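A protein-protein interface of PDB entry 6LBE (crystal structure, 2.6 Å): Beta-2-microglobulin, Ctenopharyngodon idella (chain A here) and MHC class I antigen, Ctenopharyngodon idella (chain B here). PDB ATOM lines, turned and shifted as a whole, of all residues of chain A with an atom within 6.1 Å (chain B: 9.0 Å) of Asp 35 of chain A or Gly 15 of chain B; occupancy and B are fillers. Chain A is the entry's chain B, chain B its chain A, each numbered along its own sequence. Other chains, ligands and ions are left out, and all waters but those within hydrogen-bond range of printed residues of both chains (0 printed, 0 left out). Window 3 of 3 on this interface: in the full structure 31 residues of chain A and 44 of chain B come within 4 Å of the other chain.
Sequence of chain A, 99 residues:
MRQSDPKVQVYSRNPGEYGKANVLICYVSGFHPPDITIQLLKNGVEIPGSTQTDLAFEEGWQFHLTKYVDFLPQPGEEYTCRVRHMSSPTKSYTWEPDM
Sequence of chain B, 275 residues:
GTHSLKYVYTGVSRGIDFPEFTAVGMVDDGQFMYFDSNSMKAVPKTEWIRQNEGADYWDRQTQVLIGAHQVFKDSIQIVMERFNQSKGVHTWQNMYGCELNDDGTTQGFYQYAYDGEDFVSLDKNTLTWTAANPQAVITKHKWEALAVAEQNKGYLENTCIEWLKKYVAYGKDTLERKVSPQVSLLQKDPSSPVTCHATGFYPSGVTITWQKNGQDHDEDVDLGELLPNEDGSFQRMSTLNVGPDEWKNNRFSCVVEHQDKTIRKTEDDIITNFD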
ATOM      1  N   PHE A  31      17.318  13.525  32.930  1.00  0.00           N
ATOM      2  CA  PHE A  31      17.615  13.945  31.572  1.00  0.00           C
ATOM      3  C   PHE A  31      16.509  13.463  30.642  1.00  0.00           C
ATOM      4  O   PHE A  31      15.887  12.424  30.875  1.00  0.00           O
ATOM      5  CB  PHE A  31      18.974  13.402  31.117  1.00  0.00           C
ATOM      6  CG  PHE A  31      19.115  11.908  31.288  1.00  0.00           C
ATOM      7  CD1 PHE A  31      18.659  11.031  30.307  1.00  0.00           C
ATOM      8  CD2 PHE A  31      19.678  11.378  32.437  1.00  0.00           C
ATOM      9  CE1 PHE A  31      18.768   9.674  30.470  1.00  0.00           C
ATOM     10  CE2 PHE A  31      19.792   9.996  32.603  1.00  0.00           C
ATOM     11  CZ  PHE A  31      19.333   9.153  31.623  1.00  0.00           C
ATOM     12  N   PRO A  33      15.092  13.867  26.227  1.00  0.00           N
ATOM     13  CA  PRO A  33      14.901  12.428  25.997  1.00  0.00           C
ATOM     14  C   PRO A  33      16.144  11.578  26.386  1.00  0.00           C
ATOM     15  O   PRO A  33      17.185  12.154  26.704  1.00  0.00           O
ATOM     16  CB  PRO A  33      14.627  12.369  24.484  1.00  0.00           C
ATOM     17  CG  PRO A  33      15.086  13.657  23.954  1.00  0.00           C
ATOM     18  CD  PRO A  33      14.806  14.635  25.008  1.00  0.00           C
ATOM     19  N   PRO A  34      16.041  10.242  26.335  1.00  0.00           N
ATOM     20  CA  PRO A  34      17.070   9.401  26.983  1.00  0.00           C
ATOM     21  C   PRO A  34      18.487   9.476  26.412  1.00  0.00           C
ATOM     22  O   PRO A  34      19.430   9.174  27.156  1.00  0.00           O
ATOM     23  CB  PRO A  34      16.500   7.982  26.834  1.00  0.00           C
ATOM     24  CG  PRO A  34      15.039   8.172  26.755  1.00  0.00           C
ATOM     25  CD  PRO A  34      14.851   9.448  25.978  1.00  0.00           C
ATOM     26  N   ASP A  35      18.688   9.848  25.145  1.00  0.00           N
ATOM     27  CA  ASP A  35      19.996   9.675  24.503  1.00  0.00           C
ATOM     28  C   ASP A  35      21.105  10.302  25.359  1.00  0.00           C
ATOM     29  O   ASP A  35      21.135  11.523  25.553  1.00  0.00           O
ATOM     30  CB  ASP A  35      19.945  10.241  23.087  1.00  0.00           C
ATOM     31  CG  ASP A  35      19.459   9.216  22.066  1.00  0.00           C
ATOM     32  OD1 ASP A  35      19.148   8.066  22.465  1.00  0.00           O
ATOM     33  OD2 ASP A  35      19.383   9.556  20.865  1.00  0.00           O
ATOM     34  N   ILE A  36      22.039   9.480  25.852  1.00  0.00           N
ATOM     35  CA  ILE A  36      23.040   9.933  26.814  1.00  0.00           C
ATOM     36  C   ILE A  36      24.213   8.956  26.831  1.00  0.00           C
ATOM     37  O   ILE A  36      24.055   7.756  26.598  1.00  0.00           O
ATOM     38  CB  ILE A  36      22.501  10.156  28.246  1.00  0.00           C
ATOM     39  CG1 ILE A  36      23.378  11.166  28.987  1.00  0.00           C
ATOM     40  CG2 ILE A  36      22.470   8.848  29.010  1.00  0.00           C
ATOM     41  CD1 ILE A  36      22.628  11.984  29.999  1.00  0.00           C
ATOM     42  N   THR A  37      25.399   9.485  27.139  1.00  0.00           N
ATOM     43  CA  THR A  37      26.634   8.715  27.243  1.00  0.00           C
ATOM     44  C   THR A  37      27.370   9.133  28.504  1.00  0.00           C
ATOM     45  O   THR A  37      27.402  10.322  28.845  1.00  0.00           O
ATOM     46  CB  THR A  37      27.546   8.926  26.013  1.00  0.00           C
ATOM     47  OG1 THR A  37      27.091   8.093  24.937  1.00  0.00           O
ATOM     48  CG2 THR A  37      29.001   8.583  26.334  1.00  0.00           C
ATOM     49  N   ARG A  84      27.509  13.161  28.086  1.00  0.00           N
ATOM     50  CA  ARG A  84      27.103  13.719  26.806  1.00  0.00           C
ATOM     51  C   ARG A  84      25.632  13.386  26.609  1.00  0.00           C
ATOM     52  O   ARG A  84      25.264  12.218  26.477  1.00  0.00           O
ATOM     53  CB  ARG A  84      27.968  13.169  25.673  1.00  0.00           C
ATOM     54  CG  ARG A  84      27.958  14.037  24.414  1.00  0.00           C
ATOM     55  CD  ARG A  84      26.709  13.797  23.580  1.00  0.00           C
ATOM     56  NE  ARG A  84      26.699  12.426  23.075  1.00  0.00           N
ATOM     57  CZ  ARG A  84      25.600  11.724  22.836  1.00  0.00           C
ATOM     58  NH1 ARG A  84      24.405  12.263  23.042  1.00  0.00           N
ATOM     59  NH2 ARG A  84      25.700  10.483  22.381  1.00  0.00           N
ATOM     60  N   HIS A  85      24.790  14.403  26.609  1.00  0.00           N
ATOM     61  CA  HIS A  85      23.353  14.227  26.464  1.00  0.00           C
ATOM     62  C   HIS A  85      22.896  14.838  25.145  1.00  0.00           C
ATOM     63  O   HIS A  85      23.102  16.035  24.917  1.00  0.00           O
ATOM     64  CB  HIS A  85      22.610  14.881  27.616  1.00  0.00           C
ATOM     65  CG  HIS A  85      21.123  14.794  27.494  1.00  0.00           C
ATOM     66  ND1 HIS A  85      20.302  15.896  27.587  1.00  0.00           N
ATOM     67  CD2 HIS A  85      20.305  13.728  27.314  1.00  0.00           C
ATOM     68  CE1 HIS A  85      19.041  15.512  27.473  1.00  0.00           C
ATOM     69  NE2 HIS A  85      19.017  14.202  27.304  1.00  0.00           N
ATOM     70  N   MET A  86      22.218  14.043  24.330  1.00  0.00           N
ATOM     71  CA  MET A  86      21.737  14.483  23.050  1.00  0.00           C
ATOM     72  C   MET A  86      22.891  15.010  22.222  1.00  0.00           C
ATOM     73  O   MET A  86      23.921  14.408  22.148  1.00  0.00           O
ATOM     74  CB  MET A  86      20.725  15.572  23.252  1.00  0.00           C
ATOM     75  CG  MET A  86      19.415  15.186  23.820  1.00  0.00           C
ATOM     76  SD  MET A  86      18.670  13.786  23.108  1.00  0.00           S
ATOM     77  CE  MET A  86      18.791  14.084  21.409  1.00  0.00           C
ATOM     78  N   THR B  10      10.541   1.836  28.486  1.00  0.00           N
ATOM     79  CA  THR B  10      11.008   3.052  27.822  1.00  0.00           C
ATOM     80  C   THR B  10      10.932   2.814  26.321  1.00  0.00           C
ATOM     81  O   THR B  10      11.684   1.993  25.778  1.00  0.00           O
ATOM     82  CB  THR B  10      12.436   3.390  28.233  1.00  0.00           C
ATOM     83  OG1 THR B  10      12.468   3.569  29.651  1.00  0.00           O
ATOM     84  CG2 THR B  10      12.896   4.663  27.538  1.00  0.00           C
ATOM     85  N   GLY B  11      10.040   3.523  25.646  1.00  0.00           N
ATOM     86  CA  GLY B  11       9.980   3.502  24.190  1.00  0.00           C
ATOM     87  C   GLY B  11      10.320   4.868  23.623  1.00  0.00           C
ATOM     88  O   GLY B  11       9.871   5.893  24.149  1.00  0.00           O
ATOM     89  N   VAL B  12      11.079   4.881  22.526  1.00  0.00           N
ATOM     90  CA  VAL B  12      11.602   6.135  21.979  1.00  0.00           C
ATOM     91  C   VAL B  12      11.487   6.100  20.466  1.00  0.00           C
ATOM     92  O   VAL B  12      12.051   5.212  19.817  1.00  0.00           O
ATOM     93  CB  VAL B  12      13.064   6.390  22.382  1.00  0.00           C
ATOM     94  CG1 VAL B  12      13.532   7.719  21.816  1.00  0.00           C
ATOM     95  CG2 VAL B  12      13.211   6.353  23.901  1.00  0.00           C
ATOM     96  N   SER B  13      10.787   7.080  19.901  1.00  0.00           N
ATOM     97  CA  SER B  13      10.578   7.091  18.456  1.00  0.00           C
ATOM     98  C   SER B  13      11.894   7.273  17.697  1.00  0.00           C
ATOM     99  O   SER B  13      12.261   6.433  16.864  1.00  0.00           O
ATOM    100  CB  SER B  13       9.578   8.184  18.079  1.00  0.00           C
ATOM    101  OG  SER B  13      10.082   9.465  18.418  1.00  0.00           O
ATOM    102  N   ARG B  14      12.621   8.363  17.961  1.00  0.00           N
ATOM    103  CA  ARG B  14      13.710   8.763  17.065  1.00  0.00           C
ATOM    104  C   ARG B  14      15.082   8.942  17.706  1.00  0.00           C
ATOM    105  O   ARG B  14      15.892   9.752  17.247  1.00  0.00           O
ATOM    106  CB  ARG B  14      13.338  10.009  16.256  1.00  0.00           C
ATOM    107  CG  ARG B  14      12.090   9.871  15.411  1.00  0.00           C
ATOM    108  CD  ARG B  14      12.381   9.220  14.052  1.00  0.00           C
ATOM    109  NE  ARG B  14      11.198   9.240  13.189  1.00  0.00           N
ATOM    110  CZ  ARG B  14      11.223   9.367  11.863  1.00  0.00           C
ATOM    111  NH1 ARG B  14      10.077   9.385  11.183  1.00  0.00           N
ATOM    112  NH2 ARG B  14      12.385   9.482  11.217  1.00  0.00           N
ATOM    113  N   GLY B  15      15.381   8.171  18.757  1.00  0.00           N
ATOM    114  CA  GLY B  15      16.689   8.196  19.376  1.00  0.00           C
ATOM    115  C   GLY B  15      17.796   7.442  18.652  1.00  0.00           C
ATOM    116  O   GLY B  15      17.593   6.815  17.616  1.00  0.00           O
ATOM    117  N   ILE B  16      18.988   7.490  19.246  1.00  0.00           N
ATOM    118  CA  ILE B  16      20.185   6.901  18.651  1.00  0.00           C
ATOM    119  C   ILE B  16      20.923   5.985  19.625  1.00  0.00           C
ATOM    120  O   ILE B  16      21.312   4.860  19.283  1.00  0.00           O
ATOM    121  CB  ILE B  16      21.122   8.021  18.170  1.00  0.00           C
ATOM    122  CG1 ILE B  16      20.377   8.945  17.204  1.00  0.00           C
ATOM    123  CG2 ILE B  16      22.363   7.425  17.552  1.00  0.00           C
ATOM    124  CD1 ILE B  16      21.189  10.101  16.725  1.00  0.00           C
ATOM    125  N   ASP B  17      21.154   6.477  20.839  1.00  0.00           N
ATOM    126  CA  ASP B  17      22.021   5.780  21.780  1.00  0.00           C
ATOM    127  C   ASP B  17      21.363   4.561  22.403  1.00  0.00           C
ATOM    128  O   ASP B  17      22.058   3.694  22.939  1.00  0.00           O
ATOM    129  CB  ASP B  17      22.467   6.752  22.866  1.00  0.00           C
ATOM    130  CG  ASP B  17      23.242   7.924  22.301  1.00  0.00           C
ATOM    131  OD1 ASP B  17      24.396   7.698  21.873  1.00  0.00           O
ATOM    132  OD2 ASP B  17      22.700   9.057  22.269  1.00  0.00           O
ATOM    133  N   PHE B  18      20.049   4.466  22.332  1.00  0.00           N
ATOM    134  CA  PHE B  18      19.366   3.389  23.013  1.00  0.00           C
ATOM    135  C   PHE B  18      18.457   2.659  22.045  1.00  0.00           C
ATOM    136  O   PHE B  18      18.023   3.229  21.040  1.00  0.00           O
ATOM    137  CB  PHE B  18      18.549   3.924  24.191  1.00  0.00           C
ATOM    138  CG  PHE B  18      19.384   4.253  25.382  1.00  0.00           C
ATOM    139  CD1 PHE B  18      19.974   3.241  26.119  1.00  0.00           C
ATOM    140  CD2 PHE B  18      19.597   5.570  25.758  1.00  0.00           C
ATOM    141  CE1 PHE B  18      20.760   3.535  27.214  1.00  0.00           C
ATOM    142  CE2 PHE B  18      20.372   5.864  26.849  1.00  0.00           C
ATOM    143  CZ  PHE B  18      20.956   4.843  27.574  1.00  0.00           C
ATOM    144  N   PRO B  19      18.182   1.389  22.311  1.00  0.00           N
ATOM    145  CA  PRO B  19      17.165   0.681  21.534  1.00  0.00           C
ATOM    146  C   PRO B  19      15.844   1.432  21.545  1.00  0.00           C
ATOM    147  O   PRO B  19      15.560   2.230  22.436  1.00  0.00           O
ATOM    148  CB  PRO B  19      17.059  -0.666  22.254  1.00  0.00           C
ATOM    149  CG  PRO B  19      18.471  -0.876  22.804  1.00  0.00           C
ATOM    150  CD  PRO B  19      18.912   0.492  23.227  1.00  0.00           C
ATOM    151  N   GLU B  20      15.043   1.166  20.511  1.00  0.00           N
ATOM    152  CA  GLU B  20      13.722   1.774  20.369  1.00  0.00           C
ATOM    153  C   GLU B  20      12.879   1.578  21.621  1.00  0.00           C
ATOM    154  O   GLU B  20      12.235   2.519  22.105  1.00  0.00           O
ATOM    155  CB  GLU B  20      13.019   1.162  19.153  1.00  0.00           C
ATOM    156  CG  GLU B  20      11.884   1.989  18.556  1.00  0.00           C
ATOM    157  CD  GLU B  20      11.409   1.460  17.176  1.00  0.00           C
ATOM    158  OE1 GLU B  20      11.167   2.290  16.268  1.00  0.00           O
ATOM    159  OE2 GLU B  20      11.268   0.223  16.998  1.00  0.00           O
ATOM    160  N   PHE B  21      12.885   0.354  22.161  1.00  0.00           N
ATOM    161  CA  PHE B  21      12.005  -0.079  23.241  1.00  0.00           C
ATOM    162  C   PHE B  21      12.846  -0.840  24.257  1.00  0.00           C
ATOM    163  O   PHE B  21      13.508  -1.816  23.893  1.00  0.00           O
ATOM    164  CB  PHE B  21      10.879  -0.960  22.683  1.00  0.00           C
ATOM    165  CG  PHE B  21       9.882  -1.435  23.715  1.00  0.00           C
ATOM    166  CD1 PHE B  21       8.921  -0.575  24.218  1.00  0.00           C
ATOM    167  CD2 PHE B  21       9.887  -2.752  24.148  1.00  0.00           C
ATOM    168  CE1 PHE B  21       8.008  -1.016  25.161  1.00  0.00           C
ATOM    169  CE2 PHE B  21       8.974  -3.203  25.078  1.00  0.00           C
ATOM    170  CZ  PHE B  21       8.035  -2.330  25.596  1.00  0.00           C
ATOM    171  N   PHE B  72       3.727  -0.551  21.424  1.00  0.00           N
ATOM    172  CA  PHE B  72       4.334   0.759  21.654  1.00  0.00           C
ATOM    173  C   PHE B  72       4.536   1.504  20.336  1.00  0.00           C
ATOM    174  O   PHE B  72       4.155   2.676  20.213  1.00  0.00           O
ATOM    175  CB  PHE B  72       5.679   0.655  22.381  1.00  0.00           C
ATOM    176  CG  PHE B  72       6.692   1.670  21.877  1.00  0.00           C
ATOM    177  CD1 PHE B  72       6.533   3.031  22.148  1.00  0.00           C
ATOM    178  CD2 PHE B  72       7.756   1.278  21.074  1.00  0.00           C
ATOM    179  CE1 PHE B  72       7.431   3.965  21.650  1.00  0.00           C
ATOM    180  CE2 PHE B  72       8.661   2.207  20.573  1.00  0.00           C
ATOM    181  CZ  PHE B  72       8.501   3.549  20.857  1.00  0.00           C
ATOM    182  N   ILE B  76       2.762   5.174  19.896  1.00  0.00           N
ATOM    183  CA  ILE B  76       3.402   6.489  19.924  1.00  0.00           C
ATOM    184  C   ILE B  76       3.120   7.304  18.654  1.00  0.00           C
ATOM    185  O   ILE B  76       3.100   8.539  18.704  1.00  0.00           O
ATOM    186  CB  ILE B  76       4.915   6.356  20.200  1.00  0.00           C
ATOM    187  CG1 ILE B  76       5.436   7.627  20.896  1.00  0.00           C
ATOM    188  CG2 ILE B  76       5.698   6.036  18.932  1.00  0.00           C
ATOM    189  CD1 ILE B  76       6.949   7.710  20.979  1.00  0.00           C
ATOM    190  N   GLY B  88      10.333  14.808  15.164  1.00  0.00           N
ATOM    191  CA  GLY B  88      11.116  14.720  16.363  1.00  0.00           C
ATOM    192  C   GLY B  88      11.297  13.493  17.164  1.00  0.00           C
ATOM    193  O   GLY B  88      10.815  12.468  16.786  1.00  0.00           O
ATOM    194  N   VAL B  89      12.015  13.636  18.277  1.00  0.00           N
ATOM    195  CA  VAL B  89      12.248  12.551  19.214  1.00  0.00           C
ATOM    196  C   VAL B  89      11.186  12.689  20.255  1.00  0.00           C
ATOM    197  O   VAL B  89      10.940  13.754  20.709  1.00  0.00           O
ATOM    198  CB  VAL B  89      13.610  12.623  19.885  1.00  0.00           C
ATOM    199  CG1 VAL B  89      13.839  11.380  20.687  1.00  0.00           C
ATOM    200  CG2 VAL B  89      14.683  12.812  18.866  1.00  0.00           C
ATOM    201  N   HIS B  90      10.450  11.635  20.529  1.00  0.00           N
ATOM    202  CA  HIS B  90       9.388  11.650  21.521  1.00  0.00           C
ATOM    203  C   HIS B  90       9.479  10.349  22.355  1.00  0.00           C
ATOM    204  O   HIS B  90       9.958   9.372  21.864  1.00  0.00           O
ATOM    205  CB  HIS B  90       8.008  11.840  20.842  1.00  0.00           C
ATOM    206  CG  HIS B  90       7.849  13.121  20.065  1.00  0.00           C
ATOM    207  ND1 HIS B  90       7.209  14.220  20.559  1.00  0.00           N
ATOM    208  CD2 HIS B  90       8.226  13.458  18.816  1.00  0.00           C
ATOM    209  CE1 HIS B  90       7.248  15.194  19.677  1.00  0.00           C
ATOM    210  NE2 HIS B  90       7.849  14.750  18.604  1.00  0.00           N
ATOM    211  N   THR B  91       9.048  10.337  23.611  1.00  0.00           N
ATOM    212  CA  THR B  91       9.136   9.122  24.404  1.00  0.00           C
ATOM    213  C   THR B  91       7.749   8.644  24.805  1.00  0.00           C
ATOM    214  O   THR B  91       6.841   9.447  25.067  1.00  0.00           O
ATOM    215  CB  THR B  91       9.998   9.317  25.672  1.00  0.00           C
ATOM    216  OG1 THR B  91       9.340  10.227  26.556  1.00  0.00           O
ATOM    217  CG2 THR B  91      11.350   9.873  25.314  1.00  0.00           C
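The backbone NH (N) of Ile 16 of chain B lies within hydrogen-bond range of the side-chain carboxylate (OD2) of Asp 35 of chain A, at 2.7 Å.
N of Asp 17 of chain B sits at hydrogen-bond distance from OD1 of Asp 35 of chain A (3.0 Å).
OD1 of Asp 17 of chain B is in salt-bridge range of NH2 of Arg 84 of chain A (3.1 Å).
Val 12 of chain B touches Pro 34 of chain A (CG2 to CG, 3.8 Å).
Phe 18 of chain B touches Pro 34 of chain A (CE2 to O, 3.5 Å).
Pro 34 of chain A touches Thr 91 of chain B.
CA of Gly 15 of chain B touches OD2 of Asp 35 of chain A (3.4 Å).
Phe 18 of chain B touches Asp 35 of chain A (N to OD1, 3.7 Å).
N of Ile 36 of chain A touches OD2 of Asp 17 of chain B (3.7 Å).
The backbone NH of Met 86 of chain A is in hydrogen-bond range of the backbone carbonyl oxygen of Asp 35 of chain A, at 3.0 Å.
N of Val 12 of chain B lies within hydrogen-bond range of O of Glu 20 of chain B (2.7 Å).
O of Arg 84 of chain A is in hydrogen-bond range of N of Thr 37 of chain A (2.8 Å).
Asp 35 of chain A touches four residues of chain B.
Gly 15 of chain B touches just one residue of chain A: Asp 35 (3.4 Å).
Pro 34 of chain A touches just these residues of chain B: Val 12 (3.8 Å), Phe 18 (3.5 Å) and Thr 91 (3.6 Å).
Of the printed residues of chain B, Ile 36 of chain A touches Asp 17 (3.7 Å).
Printed residues of chain A within 4 Å of Thr 91 of chain B: Pro 34.
Printed residues of chain A within 4 Å of Asp 17 of chain B: Asp 35 (3.0 Å), Ile 36 (3.7 Å) and Arg 84 (3.1 Å).
Of the printed residues of chain A, Val 12 of chain B touches Pro 34.
Printed residues of chain B that touch a printed residue of chain A: Val 12, Gly 15, Ile 16, Asp 17, Phe 18 and Thr 91.
Hydrophobic or aromatic side chains of chain B within 4 Å of the printed part of chain A: Val 12, Ile 16 and Phe 18.
Along chain B the printed residues that touch a printed residue of chain A span positions 12 to 91.
Printed residues of chain A that touch a printed residue of chain B: Pro 34, Asp 35, Ile 36 and Arg 84.
Hydrophobic or aromatic side chains of chain A that line the printed part of chain B: Pro 34.
Among the printed residues, Asp or Glu carboxylates within 4 Å of a Lys or Arg side-chain nitrogen of the other chain: Arg 84 of chain A with Asp 17 of chain B (3.1 Å).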
